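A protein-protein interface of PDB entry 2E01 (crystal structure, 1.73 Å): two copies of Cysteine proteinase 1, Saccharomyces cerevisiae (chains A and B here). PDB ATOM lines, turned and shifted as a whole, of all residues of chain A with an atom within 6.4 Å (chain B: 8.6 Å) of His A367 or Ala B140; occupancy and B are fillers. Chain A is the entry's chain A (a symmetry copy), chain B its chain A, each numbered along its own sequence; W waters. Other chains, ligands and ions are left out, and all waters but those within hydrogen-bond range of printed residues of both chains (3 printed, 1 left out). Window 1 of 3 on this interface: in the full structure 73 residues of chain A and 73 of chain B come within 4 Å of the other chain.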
ATOM      1  N   SER A 362      12.807 -15.811 -38.885  1.00  0.00           N
ATOM      2  CA  SER A 362      12.948 -16.070 -37.467  1.00  0.00           C
ATOM      3  C   SER A 362      12.735 -14.803 -36.638  1.00  0.00           C
ATOM      4  O   SER A 362      12.227 -14.899 -35.526  1.00  0.00           O
ATOM      5  CB  SER A 362      14.336 -16.696 -37.151  1.00  0.00           C
ATOM      6  OG  SER A 362      14.416 -17.973 -37.765  1.00  0.00           O
ATOM      7  N   ARG A 363      13.123 -13.642 -37.165  1.00  0.00           N
ATOM      8  CA  ARG A 363      12.898 -12.394 -36.420  1.00  0.00           C
ATOM      9  C   ARG A 363      11.391 -12.266 -36.196  1.00  0.00           C
ATOM     10  O   ARG A 363      10.933 -11.818 -35.152  1.00  0.00           O
ATOM     11  CB  ARG A 363      13.327 -11.176 -37.231  1.00  0.00           C
ATOM     12  CG  ARG A 363      14.831 -10.995 -37.416  1.00  0.00           C
ATOM     13  CD  ARG A 363      15.079 -10.052 -38.599  1.00  0.00           C
ATOM     14  NE  ARG A 363      16.303 -10.417 -39.300  1.00  0.00           N
ATOM     15  CZ  ARG A 363      16.612 -10.048 -40.536  1.00  0.00           C
ATOM     16  NH1 ARG A 363      15.780  -9.277 -41.240  1.00  0.00           N
ATOM     17  NH2 ARG A 363      17.751 -10.481 -41.073  1.00  0.00           N
ATOM     18  N   ILE A 364      10.619 -12.639 -37.209  1.00  0.00           N
ATOM     19  CA  ILE A 364       9.157 -12.536 -37.080  1.00  0.00           C
ATOM     20  C   ILE A 364       8.619 -13.528 -36.062  1.00  0.00           C
ATOM     21  O   ILE A 364       7.851 -13.154 -35.140  1.00  0.00           O
ATOM     22  CB  ILE A 364       8.458 -12.745 -38.437  1.00  0.00           C
ATOM     23  CG1 ILE A 364       8.874 -11.660 -39.414  1.00  0.00           C
ATOM     24  CG2 ILE A 364       6.912 -12.722 -38.223  1.00  0.00           C
ATOM     25  CD1 ILE A 364       8.417 -11.941 -40.849  1.00  0.00           C
ATOM     26  N   ARG A 365       9.065 -14.796 -36.159  1.00  0.00           N
ATOM     27  CA  ARG A 365       8.590 -15.821 -35.233  1.00  0.00           C
ATOM     28  C   ARG A 365       8.983 -15.603 -33.794  1.00  0.00           C
ATOM     29  O   ARG A 365       8.212 -15.903 -32.872  1.00  0.00           O
ATOM     30  CB  ARG A 365       9.097 -17.204 -35.618  1.00  0.00           C
ATOM     31  CG  ARG A 365       8.374 -17.763 -36.826  1.00  0.00           C
ATOM     32  CD  ARG A 365       8.625 -19.242 -36.847  1.00  0.00           C
ATOM     33  NE  ARG A 365       9.328 -19.547 -38.076  1.00  0.00           N
ATOM     34  CZ  ARG A 365       8.721 -19.921 -39.177  1.00  0.00           C
ATOM     35  NH1 ARG A 365       7.398 -20.062 -39.180  1.00  0.00           N
ATOM     36  NH2 ARG A 365       9.425 -20.096 -40.272  1.00  0.00           N
ATOM     37  N   TYR A 366      10.179 -15.021 -33.633  1.00  0.00           N
ATOM     38  CA  TYR A 366      10.721 -14.818 -32.303  1.00  0.00           C
ATOM     39  C   TYR A 366      10.447 -13.489 -31.657  1.00  0.00           C
ATOM     40  O   TYR A 366      11.117 -13.145 -30.690  1.00  0.00           O
ATOM     41  CB  TYR A 366      12.229 -15.163 -32.249  1.00  0.00           C
ATOM     42  CG  TYR A 366      12.439 -16.668 -32.166  1.00  0.00           C
ATOM     43  CD1 TYR A 366      12.305 -17.459 -33.286  1.00  0.00           C
ATOM     44  CD2 TYR A 366      12.680 -17.297 -30.936  1.00  0.00           C
ATOM     45  CE1 TYR A 366      12.402 -18.864 -33.195  1.00  0.00           C
ATOM     46  CE2 TYR A 366      12.774 -18.705 -30.834  1.00  0.00           C
ATOM     47  CZ  TYR A 366      12.636 -19.471 -31.969  1.00  0.00           C
ATOM     48  OH  TYR A 366      12.714 -20.872 -31.911  1.00  0.00           O
ATOM     49  N   HIS A 367       9.400 -12.789 -32.126  1.00  0.00           N
ATOM     50  CA  HIS A 367       8.954 -11.536 -31.493  1.00  0.00           C
ATOM     51  C   HIS A 367       9.885 -10.358 -31.652  1.00  0.00           C
ATOM     52  O   HIS A 367       9.745  -9.355 -30.943  1.00  0.00           O
ATOM     53  CB  HIS A 367       8.702 -11.789 -30.004  1.00  0.00           C
ATOM     54  CG  HIS A 367       7.558 -11.013 -29.410  1.00  0.00           C
ATOM     55  ND1 HIS A 367       7.518  -9.629 -29.369  1.00  0.00           N
ATOM     56  CD2 HIS A 367       6.444 -11.438 -28.759  1.00  0.00           C
ATOM     57  CE1 HIS A 367       6.432  -9.241 -28.720  1.00  0.00           C
ATOM     58  NE2 HIS A 367       5.765 -10.320 -28.337  1.00  0.00           N
ATOM     59  N   GLU A 368      10.786 -10.447 -32.612  1.00  0.00           N
ATOM     60  CA  GLU A 368      11.725  -9.386 -32.827  1.00  0.00           C
ATOM     61  C   GLU A 368      11.301  -8.367 -33.885  1.00  0.00           C
ATOM     62  O   GLU A 368      11.594  -7.180 -33.737  1.00  0.00           O
ATOM     63  CB  GLU A 368      13.092  -9.978 -33.192  1.00  0.00           C
ATOM     64  CG  GLU A 368      14.151  -8.919 -33.560  1.00  0.00           C
ATOM     65  CD  GLU A 368      14.429  -7.857 -32.446  1.00  0.00           C
ATOM     66  OE1 GLU A 368      14.151  -8.103 -31.255  1.00  0.00           O
ATOM     67  OE2 GLU A 368      14.944  -6.772 -32.790  1.00  0.00           O
ATOM     68  N   SER A 369      10.627  -8.806 -34.955  1.00  0.00           N
ATOM     69  CA  SER A 369      10.251  -7.834 -35.981  1.00  0.00           C
ATOM     70  C   SER A 369       8.795  -8.031 -36.392  1.00  0.00           C
ATOM     71  O   SER A 369       8.281  -9.141 -36.380  1.00  0.00           O
ATOM     72  CB  SER A 369      11.179  -7.939 -37.191  1.00  0.00           C
ATOM     73  OG  SER A 369      11.071  -6.771 -37.975  1.00  0.00           O
ATOM     74  N   LEU A 370       8.144  -6.925 -36.737  1.00  0.00           N
ATOM     75  CA  LEU A 370       6.733  -6.961 -37.097  1.00  0.00           C
ATOM     76  C   LEU A 370       6.424  -5.686 -37.863  1.00  0.00           C
ATOM     77  O   LEU A 370       7.240  -4.776 -37.938  1.00  0.00           O
ATOM     78  CB  LEU A 370       5.897  -6.992 -35.809  1.00  0.00           C
ATOM     79  CG  LEU A 370       5.742  -5.673 -35.018  1.00  0.00           C
ATOM     80  CD1 LEU A 370       4.682  -5.816 -33.906  1.00  0.00           C
ATOM     81  CD2 LEU A 370       7.110  -5.208 -34.423  1.00  0.00           C
ATOM     82  N   PHE B 118      15.669 -16.030 -18.196  1.00  0.00           N
ATOM     83  CA  PHE B 118      14.984 -16.185 -19.480  1.00  0.00           C
ATOM     84  C   PHE B 118      15.551 -17.394 -20.256  1.00  0.00           C
ATOM     85  O   PHE B 118      14.784 -18.169 -20.825  1.00  0.00           O
ATOM     86  CB  PHE B 118      15.143 -14.886 -20.300  1.00  0.00           C
ATOM     87  CG  PHE B 118      14.836 -15.043 -21.761  1.00  0.00           C
ATOM     88  CD1 PHE B 118      13.514 -14.921 -22.228  1.00  0.00           C
ATOM     89  CD2 PHE B 118      15.860 -15.311 -22.680  1.00  0.00           C
ATOM     90  CE1 PHE B 118      13.214 -15.061 -23.628  1.00  0.00           C
ATOM     91  CE2 PHE B 118      15.563 -15.464 -24.110  1.00  0.00           C
ATOM     92  CZ  PHE B 118      14.249 -15.335 -24.568  1.00  0.00           C
ATOM     93  N   ILE B 122      13.358 -20.578 -21.520  1.00  0.00           N
ATOM     94  CA  ILE B 122      13.280 -21.029 -22.886  1.00  0.00           C
ATOM     95  C   ILE B 122      13.616 -22.522 -22.950  1.00  0.00           C
ATOM     96  O   ILE B 122      12.960 -23.302 -23.671  1.00  0.00           O
ATOM     97  CB  ILE B 122      14.246 -20.223 -23.806  1.00  0.00           C
ATOM     98  CG1 ILE B 122      13.716 -18.787 -23.984  1.00  0.00           C
ATOM     99  CG2 ILE B 122      14.397 -20.895 -25.152  1.00  0.00           C
ATOM    100  CD1 ILE B 122      12.339 -18.702 -24.719  1.00  0.00           C
ATOM    101  N   ILE B 130       6.717 -22.561 -31.043  1.00  0.00           N
ATOM    102  CA  ILE B 130       7.223 -21.183 -31.016  1.00  0.00           C
ATOM    103  C   ILE B 130       6.052 -20.177 -30.870  1.00  0.00           C
ATOM    104  O   ILE B 130       6.167 -19.172 -30.178  1.00  0.00           O
ATOM    105  CB  ILE B 130       8.052 -20.894 -32.296  1.00  0.00           C
ATOM    106  CG1 ILE B 130       8.568 -19.445 -32.320  1.00  0.00           C
ATOM    107  CG2 ILE B 130       7.179 -21.158 -33.564  1.00  0.00           C
ATOM    108  CD1 ILE B 130       9.301 -19.012 -31.032  1.00  0.00           C
ATOM    109  N   SER B 132       3.278 -20.673 -29.236  1.00  0.00           N
ATOM    110  CA  SER B 132       2.455 -20.957 -28.071  1.00  0.00           C
ATOM    111  C   SER B 132       2.349 -19.700 -27.210  1.00  0.00           C
ATOM    112  O   SER B 132       3.178 -18.754 -27.297  1.00  0.00           O
ATOM    113  CB  SER B 132       3.070 -22.082 -27.244  1.00  0.00           C
ATOM    114  OG  SER B 132       4.325 -21.660 -26.745  1.00  0.00           O
ATOM    115  N   ARG B 133       1.316 -19.677 -26.392  1.00  0.00           N
ATOM    116  CA  ARG B 133       1.073 -18.535 -25.545  1.00  0.00           C
ATOM    117  C   ARG B 133       2.259 -18.258 -24.587  1.00  0.00           C
ATOM    118  O   ARG B 133       2.698 -17.137 -24.461  1.00  0.00           O
ATOM    119  CB  ARG B 133      -0.216 -18.758 -24.761  1.00  0.00           C
ATOM    120  CG  ARG B 133      -0.704 -17.531 -24.036  1.00  0.00           C
ATOM    121  CD  ARG B 133      -2.037 -17.844 -23.395  1.00  0.00           C
ATOM    122  NE  ARG B 133      -2.647 -16.627 -22.887  1.00  0.00           N
ATOM    123  CZ  ARG B 133      -3.772 -16.621 -22.198  1.00  0.00           C
ATOM    124  NH1 ARG B 133      -4.398 -17.788 -21.946  1.00  0.00           N
ATOM    125  NH2 ARG B 133      -4.269 -15.470 -21.773  1.00  0.00           N
ATOM    126  N   LEU B 134       2.796 -19.290 -23.950  1.00  0.00           N
ATOM    127  CA  LEU B 134       3.918 -19.069 -23.041  1.00  0.00           C
ATOM    128  C   LEU B 134       5.205 -18.643 -23.765  1.00  0.00           C
ATOM    129  O   LEU B 134       5.881 -17.704 -23.315  1.00  0.00           O
ATOM    130  CB  LEU B 134       4.206 -20.350 -22.249  1.00  0.00           C
ATOM    131  CG  LEU B 134       5.433 -20.258 -21.335  1.00  0.00           C
ATOM    132  CD1 LEU B 134       5.298 -19.149 -20.252  1.00  0.00           C
ATOM    133  CD2 LEU B 134       5.604 -21.645 -20.670  1.00  0.00           C
ATOM    134  N   VAL B 135       5.567 -19.310 -24.858  1.00  0.00           N
ATOM    135  CA  VAL B 135       6.838 -18.947 -25.489  1.00  0.00           C
ATOM    136  C   VAL B 135       6.773 -17.518 -26.034  1.00  0.00           C
ATOM    137  O   VAL B 135       7.728 -16.766 -25.908  1.00  0.00           O
ATOM    138  CB  VAL B 135       7.246 -19.946 -26.577  1.00  0.00           C
ATOM    139  CG1 VAL B 135       8.505 -19.463 -27.308  1.00  0.00           C
ATOM    140  CG2 VAL B 135       7.471 -21.358 -25.926  1.00  0.00           C
ATOM    141  N   GLN B 136       5.651 -17.144 -26.656  1.00  0.00           N
ATOM    142  CA  GLN B 136       5.539 -15.771 -27.093  1.00  0.00           C
ATOM    143  C   GLN B 136       5.593 -14.783 -25.947  1.00  0.00           C
ATOM    144  O   GLN B 136       6.183 -13.696 -26.100  1.00  0.00           O
ATOM    145  CB  GLN B 136       4.237 -15.572 -27.883  1.00  0.00           C
ATOM    146  CG  GLN B 136       4.330 -16.241 -29.207  1.00  0.00           C
ATOM    147  CD  GLN B 136       5.400 -15.601 -30.064  1.00  0.00           C
ATOM    148  OE1 GLN B 136       5.380 -14.398 -30.309  1.00  0.00           O
ATOM    149  NE2 GLN B 136       6.339 -16.395 -30.516  1.00  0.00           N
ATOM    150  N   TYR B 137       4.989 -15.121 -24.800  1.00  0.00           N
ATOM    151  CA  TYR B 137       4.997 -14.224 -23.649  1.00  0.00           C
ATOM    152  C   TYR B 137       6.447 -14.090 -23.169  1.00  0.00           C
ATOM    153  O   TYR B 137       6.916 -12.999 -22.862  1.00  0.00           O
ATOM    154  CB  TYR B 137       4.118 -14.757 -22.486  1.00  0.00           C
ATOM    155  CG  TYR B 137       4.054 -13.795 -21.330  1.00  0.00           C
ATOM    156  CD1 TYR B 137       3.284 -12.627 -21.411  1.00  0.00           C
ATOM    157  CD2 TYR B 137       4.823 -14.011 -20.183  1.00  0.00           C
ATOM    158  CE1 TYR B 137       3.293 -11.692 -20.358  1.00  0.00           C
ATOM    159  CE2 TYR B 137       4.845 -13.098 -19.148  1.00  0.00           C
ATOM    160  CZ  TYR B 137       4.086 -11.947 -19.239  1.00  0.00           C
ATOM    161  OH  TYR B 137       4.169 -11.045 -18.224  1.00  0.00           O
ATOM    162  N   LEU B 138       7.160 -15.209 -23.100  1.00  0.00           N
ATOM    163  CA  LEU B 138       8.560 -15.127 -22.631  1.00  0.00           C
ATOM    164  C   LEU B 138       9.390 -14.182 -23.515  1.00  0.00           C
ATOM    165  O   LEU B 138      10.256 -13.407 -23.008  1.00  0.00           O
ATOM    166  CB  LEU B 138       9.205 -16.530 -22.625  1.00  0.00           C
ATOM    167  CG  LEU B 138       8.637 -17.449 -21.539  1.00  0.00           C
ATOM    168  CD1 LEU B 138       9.187 -18.886 -21.774  1.00  0.00           C
ATOM    169  CD2 LEU B 138       9.032 -16.989 -20.149  1.00  0.00           C
ATOM    170  N   LEU B 139       9.129 -14.234 -24.819  1.00  0.00           N
ATOM    171  CA  LEU B 139       9.875 -13.435 -25.803  1.00  0.00           C
ATOM    172  C   LEU B 139       9.470 -11.955 -25.846  1.00  0.00           C
ATOM    173  O   LEU B 139      10.172 -11.138 -26.391  1.00  0.00           O
ATOM    174  CB  LEU B 139       9.670 -14.050 -27.182  1.00  0.00           C
ATOM    175  CG  LEU B 139      10.277 -15.475 -27.351  1.00  0.00           C
ATOM    176  CD1 LEU B 139       9.768 -16.114 -28.687  1.00  0.00           C
ATOM    177  CD2 LEU B 139      11.791 -15.375 -27.408  1.00  0.00           C
ATOM    178  N   ALA B 140       8.342 -11.628 -25.238  1.00  0.00           N
ATOM    179  CA  ALA B 140       7.828 -10.249 -25.336  1.00  0.00           C
ATOM    180  C   ALA B 140       8.678  -9.169 -24.654  1.00  0.00           C
ATOM    181  O   ALA B 140       8.971  -8.146 -25.277  1.00  0.00           O
ATOM    182  CB  ALA B 140       6.395 -10.210 -24.776  1.00  0.00           C
ATOM    183  N   ALA B 141       9.079  -9.381 -23.405  1.00  0.00           N
ATOM    184  CA  ALA B 141       9.869  -8.364 -22.669  1.00  0.00           C
ATOM    185  C   ALA B 141      10.666  -8.999 -21.548  1.00  0.00           C
ATOM    186  O   ALA B 141      10.428  -8.712 -20.380  1.00  0.00           O
ATOM    187  CB  ALA B 141       8.911  -7.278 -22.069  1.00  0.00           C
ATOM    188  N   PRO B 142      11.643  -9.851 -21.898  1.00  0.00           N
ATOM    189  CA  PRO B 142      12.493 -10.556 -20.914  1.00  0.00           C
ATOM    190  C   PRO B 142      13.403  -9.741 -20.011  1.00  0.00           C
ATOM    191  O   PRO B 142      13.807 -10.248 -18.977  1.00  0.00           O
ATOM    192  CB  PRO B 142      13.306 -11.526 -21.780  1.00  0.00           C
ATOM    193  CG  PRO B 142      13.469 -10.820 -23.080  1.00  0.00           C
ATOM    194  CD  PRO B 142      12.017 -10.200 -23.277  1.00  0.00           C
ATOM    195  N   THR B 143      13.763  -8.519 -20.377  1.00  0.00           N
ATOM    196  CA  THR B 143      14.661  -7.778 -19.463  1.00  0.00           C
ATOM    197  C   THR B 143      14.144  -6.410 -18.971  1.00  0.00           C
ATOM    198  O   THR B 143      14.915  -5.481 -18.811  1.00  0.00           O
ATOM    199  CB  THR B 143      16.079  -7.634 -20.082  1.00  0.00           C
ATOM    200  OG1 THR B 143      16.038  -6.809 -21.253  1.00  0.00           O
ATOM    201  CG2 THR B 143      16.574  -9.030 -20.544  1.00  0.00           C
ATOM    202  N   GLU B 144      12.839  -6.315 -18.730  1.00  0.00           N
ATOM    203  CA  GLU B 144      12.298  -5.039 -18.282  1.00  0.00           C
ATOM    204  C   GLU B 144      12.717  -4.753 -16.853  1.00  0.00           C
ATOM    205  O   GLU B 144      13.165  -5.656 -16.113  1.00  0.00           O
ATOM    206  CB  GLU B 144      10.770  -4.987 -18.458  1.00  0.00           C
ATOM    207  CG  GLU B 144      10.369  -4.990 -19.930  1.00  0.00           C
ATOM    208  CD  GLU B 144      11.072  -3.878 -20.733  1.00  0.00           C
ATOM    209  OE1 GLU B 144      10.837  -2.683 -20.424  1.00  0.00           O
ATOM    210  OE2 GLU B 144      11.869  -4.202 -21.654  1.00  0.00           O
ATOM    211  N   ASN B 181      17.911  -2.093 -22.891  1.00  0.00           N
ATOM    212  CA  ASN B 181      17.002  -3.247 -22.808  1.00  0.00           C
ATOM    213  C   ASN B 181      16.642  -3.821 -24.186  1.00  0.00           C
ATOM    214  O   ASN B 181      16.534  -5.026 -24.385  1.00  0.00           O
ATOM    215  CB  ASN B 181      15.704  -2.889 -22.093  1.00  0.00           C
ATOM    216  CG  ASN B 181      15.870  -2.779 -20.629  1.00  0.00           C
ATOM    217  OD1 ASN B 181      16.752  -3.421 -20.070  1.00  0.00           O
ATOM    218  ND2 ASN B 181      14.997  -1.986 -19.959  1.00  0.00           N
ATOM    219  N   THR B 185      17.457  -7.485 -25.385  1.00  0.00           N
ATOM    220  CA  THR B 185      16.330  -8.306 -25.776  1.00  0.00           C
ATOM    221  C   THR B 185      16.482  -8.854 -27.183  1.00  0.00           C
ATOM    222  O   THR B 185      16.140 -10.018 -27.433  1.00  0.00           O
ATOM    223  CB  THR B 185      15.029  -7.495 -25.622  1.00  0.00           C
ATOM    224  OG1 THR B 185      14.854  -7.213 -24.216  1.00  0.00           O
ATOM    225  CG2 THR B 185      13.794  -8.320 -26.127  1.00  0.00           C
ATOM    226  N   THR B 186      16.999  -8.056 -28.115  1.00  0.00           N
ATOM    227  CA  THR B 186      17.176  -8.551 -29.482  1.00  0.00           C
ATOM    228  C   THR B 186      18.125  -9.745 -29.477  1.00  0.00           C
ATOM    229  O   THR B 186      17.917 -10.717 -30.176  1.00  0.00           O
ATOM    230  CB  THR B 186      17.723  -7.459 -30.402  1.00  0.00           C
ATOM    231  OG1 THR B 186      16.722  -6.460 -30.492  1.00  0.00           O
ATOM    232  CG2 THR B 186      18.020  -7.976 -31.818  1.00  0.00           C
ATOM    233  N   ARG B 189      16.419 -12.849 -28.030  1.00  0.00           N
ATOM    234  CA  ARG B 189      15.488 -13.518 -28.964  1.00  0.00           C
ATOM    235  C   ARG B 189      16.271 -14.378 -29.965  1.00  0.00           C
ATOM    236  O   ARG B 189      15.801 -15.445 -30.387  1.00  0.00           O
ATOM    237  CB  ARG B 189      14.622 -12.452 -29.675  1.00  0.00           C
ATOM    238  CG  ARG B 189      13.625 -11.880 -28.715  1.00  0.00           C
ATOM    239  CD  ARG B 189      12.924 -10.669 -29.372  1.00  0.00           C
ATOM    240  NE  ARG B 189      11.909 -10.088 -28.495  1.00  0.00           N
ATOM    241  CZ  ARG B 189      11.524  -8.803 -28.529  1.00  0.00           C
ATOM    242  NH1 ARG B 189      12.079  -7.954 -29.370  1.00  0.00           N
ATOM    243  NH2 ARG B 189      10.511  -8.398 -27.764  1.00  0.00           N
ATOM    244  N   GLU B 190      17.451 -13.900 -30.344  1.00  0.00           N
ATOM    245  CA  GLU B 190      18.352 -14.678 -31.194  1.00  0.00           C
ATOM    246  C   GLU B 190      18.760 -15.976 -30.421  1.00  0.00           C
ATOM    247  O   GLU B 190      18.694 -17.103 -30.959  1.00  0.00           O
ATOM    248  CB  GLU B 190      19.610 -13.870 -31.468  1.00  0.00           C
ATOM    249  CG  GLU B 190      20.688 -14.700 -32.232  1.00  0.00           C
ATOM    250  CD  GLU B 190      22.060 -14.061 -32.140  1.00  0.00           C
ATOM    251  OE1 GLU B 190      22.124 -12.817 -32.334  1.00  0.00           O
ATOM    252  OE2 GLU B 190      23.069 -14.795 -31.900  1.00  0.00           O
HETATM  253  O   HOH W   1      14.364  -5.518 -28.953  1.00  0.00           O
HETATM  254  O   HOH W   2       5.615 -17.013 -33.685  1.00  0.00           O
HETATM  255  O   HOH W   3      11.422  -5.539 -31.372  1.00  0.00           O
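OG1 of Thr B186 is in hydrogen-bond range of OE2 of Glu A368 (2.9 Å). The backbone carbonyl oxygen (O) of His A367 sits close to the guanidinium group (NH1) of Arg B189 (3.1 Å). The side-chain carboxylate (OE1) of Glu A368 lies within salt-bridge range of the guanidinium group (NH1) of Arg B189, at 2.8 Å. The side-chain amide nitrogen of Gln B136 is in hydrogen-bond range of the backbone carbonyl oxygen of Arg A365 (3.0 Å).
O of Ala B140 is in hydrogen-bond range of NH2 of Arg B189 (2.9 Å). The backbone NH (N) of Glu A368 sits at hydrogen-bond distance from the backbone carbonyl oxygen (O) of Arg A363 (2.9 Å). The side-chain amide nitrogen of Gln B136 lies within hydrogen-bond range of the backbone carbonyl oxygen of Ile B130, 2.8 Å away. The backbone carbonyl oxygen (O) of Leu B139 is in hydrogen-bond range of the guanidinium group (NE) of Arg B189 (2.9 Å).
Ile B130 touches Arg A365. Ile B130 touches Tyr A366 (CD1 to CE2, 3.5 Å). Leu B139 touches Tyr A366. CD of Arg B189 touches O of Tyr A366, at 3.3 Å. O of Gln B136 touches CD2 of His A367 (3.5 Å). His A367 touches Leu B139 (CB to CB, 3.7 Å). Ala B140 touches His A367 (CB to NE2, 3.6 Å).
Of chain B, only Gln B136, Leu B139, Ala B140 and Arg B189 come within 4 Å of His A367. Ala B140 touches just one residue of chain A: His A367. Of the printed residues of chain B, Glu A368 touches Thr B186 (2.9 Å) and Arg B189 (2.8 Å). Printed residues of chain A within 4 Å of Ile B130: Arg A365 (3.6 Å) and Tyr A366 (3.5 Å). Of the printed residues of chain A, Arg B189 touches Tyr A366, His A367 and Glu A368. Of the printed residues of chain B, Tyr A366 touches Ile B130, Leu B139 and Arg B189. Thr B185 touches none of the printed residues of chain A. The nearest printed residue of chain B that does not touch Tyr A366 is Gln B136 (5.0 Å).
Printed residues of chain B that touch a printed residue of chain A: Ile B130, Gln B136, Leu B139, Ala B140, Thr B186 and Arg B189. Among the printed residues, 11 pairs touch across the chains. Among the printed residues, Asp or Glu carboxylates within 4 Å of a Lys or Arg side-chain nitrogen of the other chain: Glu A368 with Arg B189.
No position is printed for both chains. Of the 11 pairs that touch across the chains among the printed residues, none has its exchanged pair printed and touching as well.
Water W3 bridges the backbone carbonyl oxygen (O) of Glu A368 (2.9 Å) and the guanidinium group (NH1) of Arg B189 (3.2 Å). Water W2 bridges the backbone carbonyl oxygen (O) of Arg A365 (2.9 Å) and the side-chain amide nitrogen (NE2) of Gln B136 (3.3 Å). Water W1 lies within hydrogen-bond range of OG1 of Thr B186 (3.0 Å), NH1 of Arg B189 (3.4 Å) and OE1 of Glu A368 (3.5 Å).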
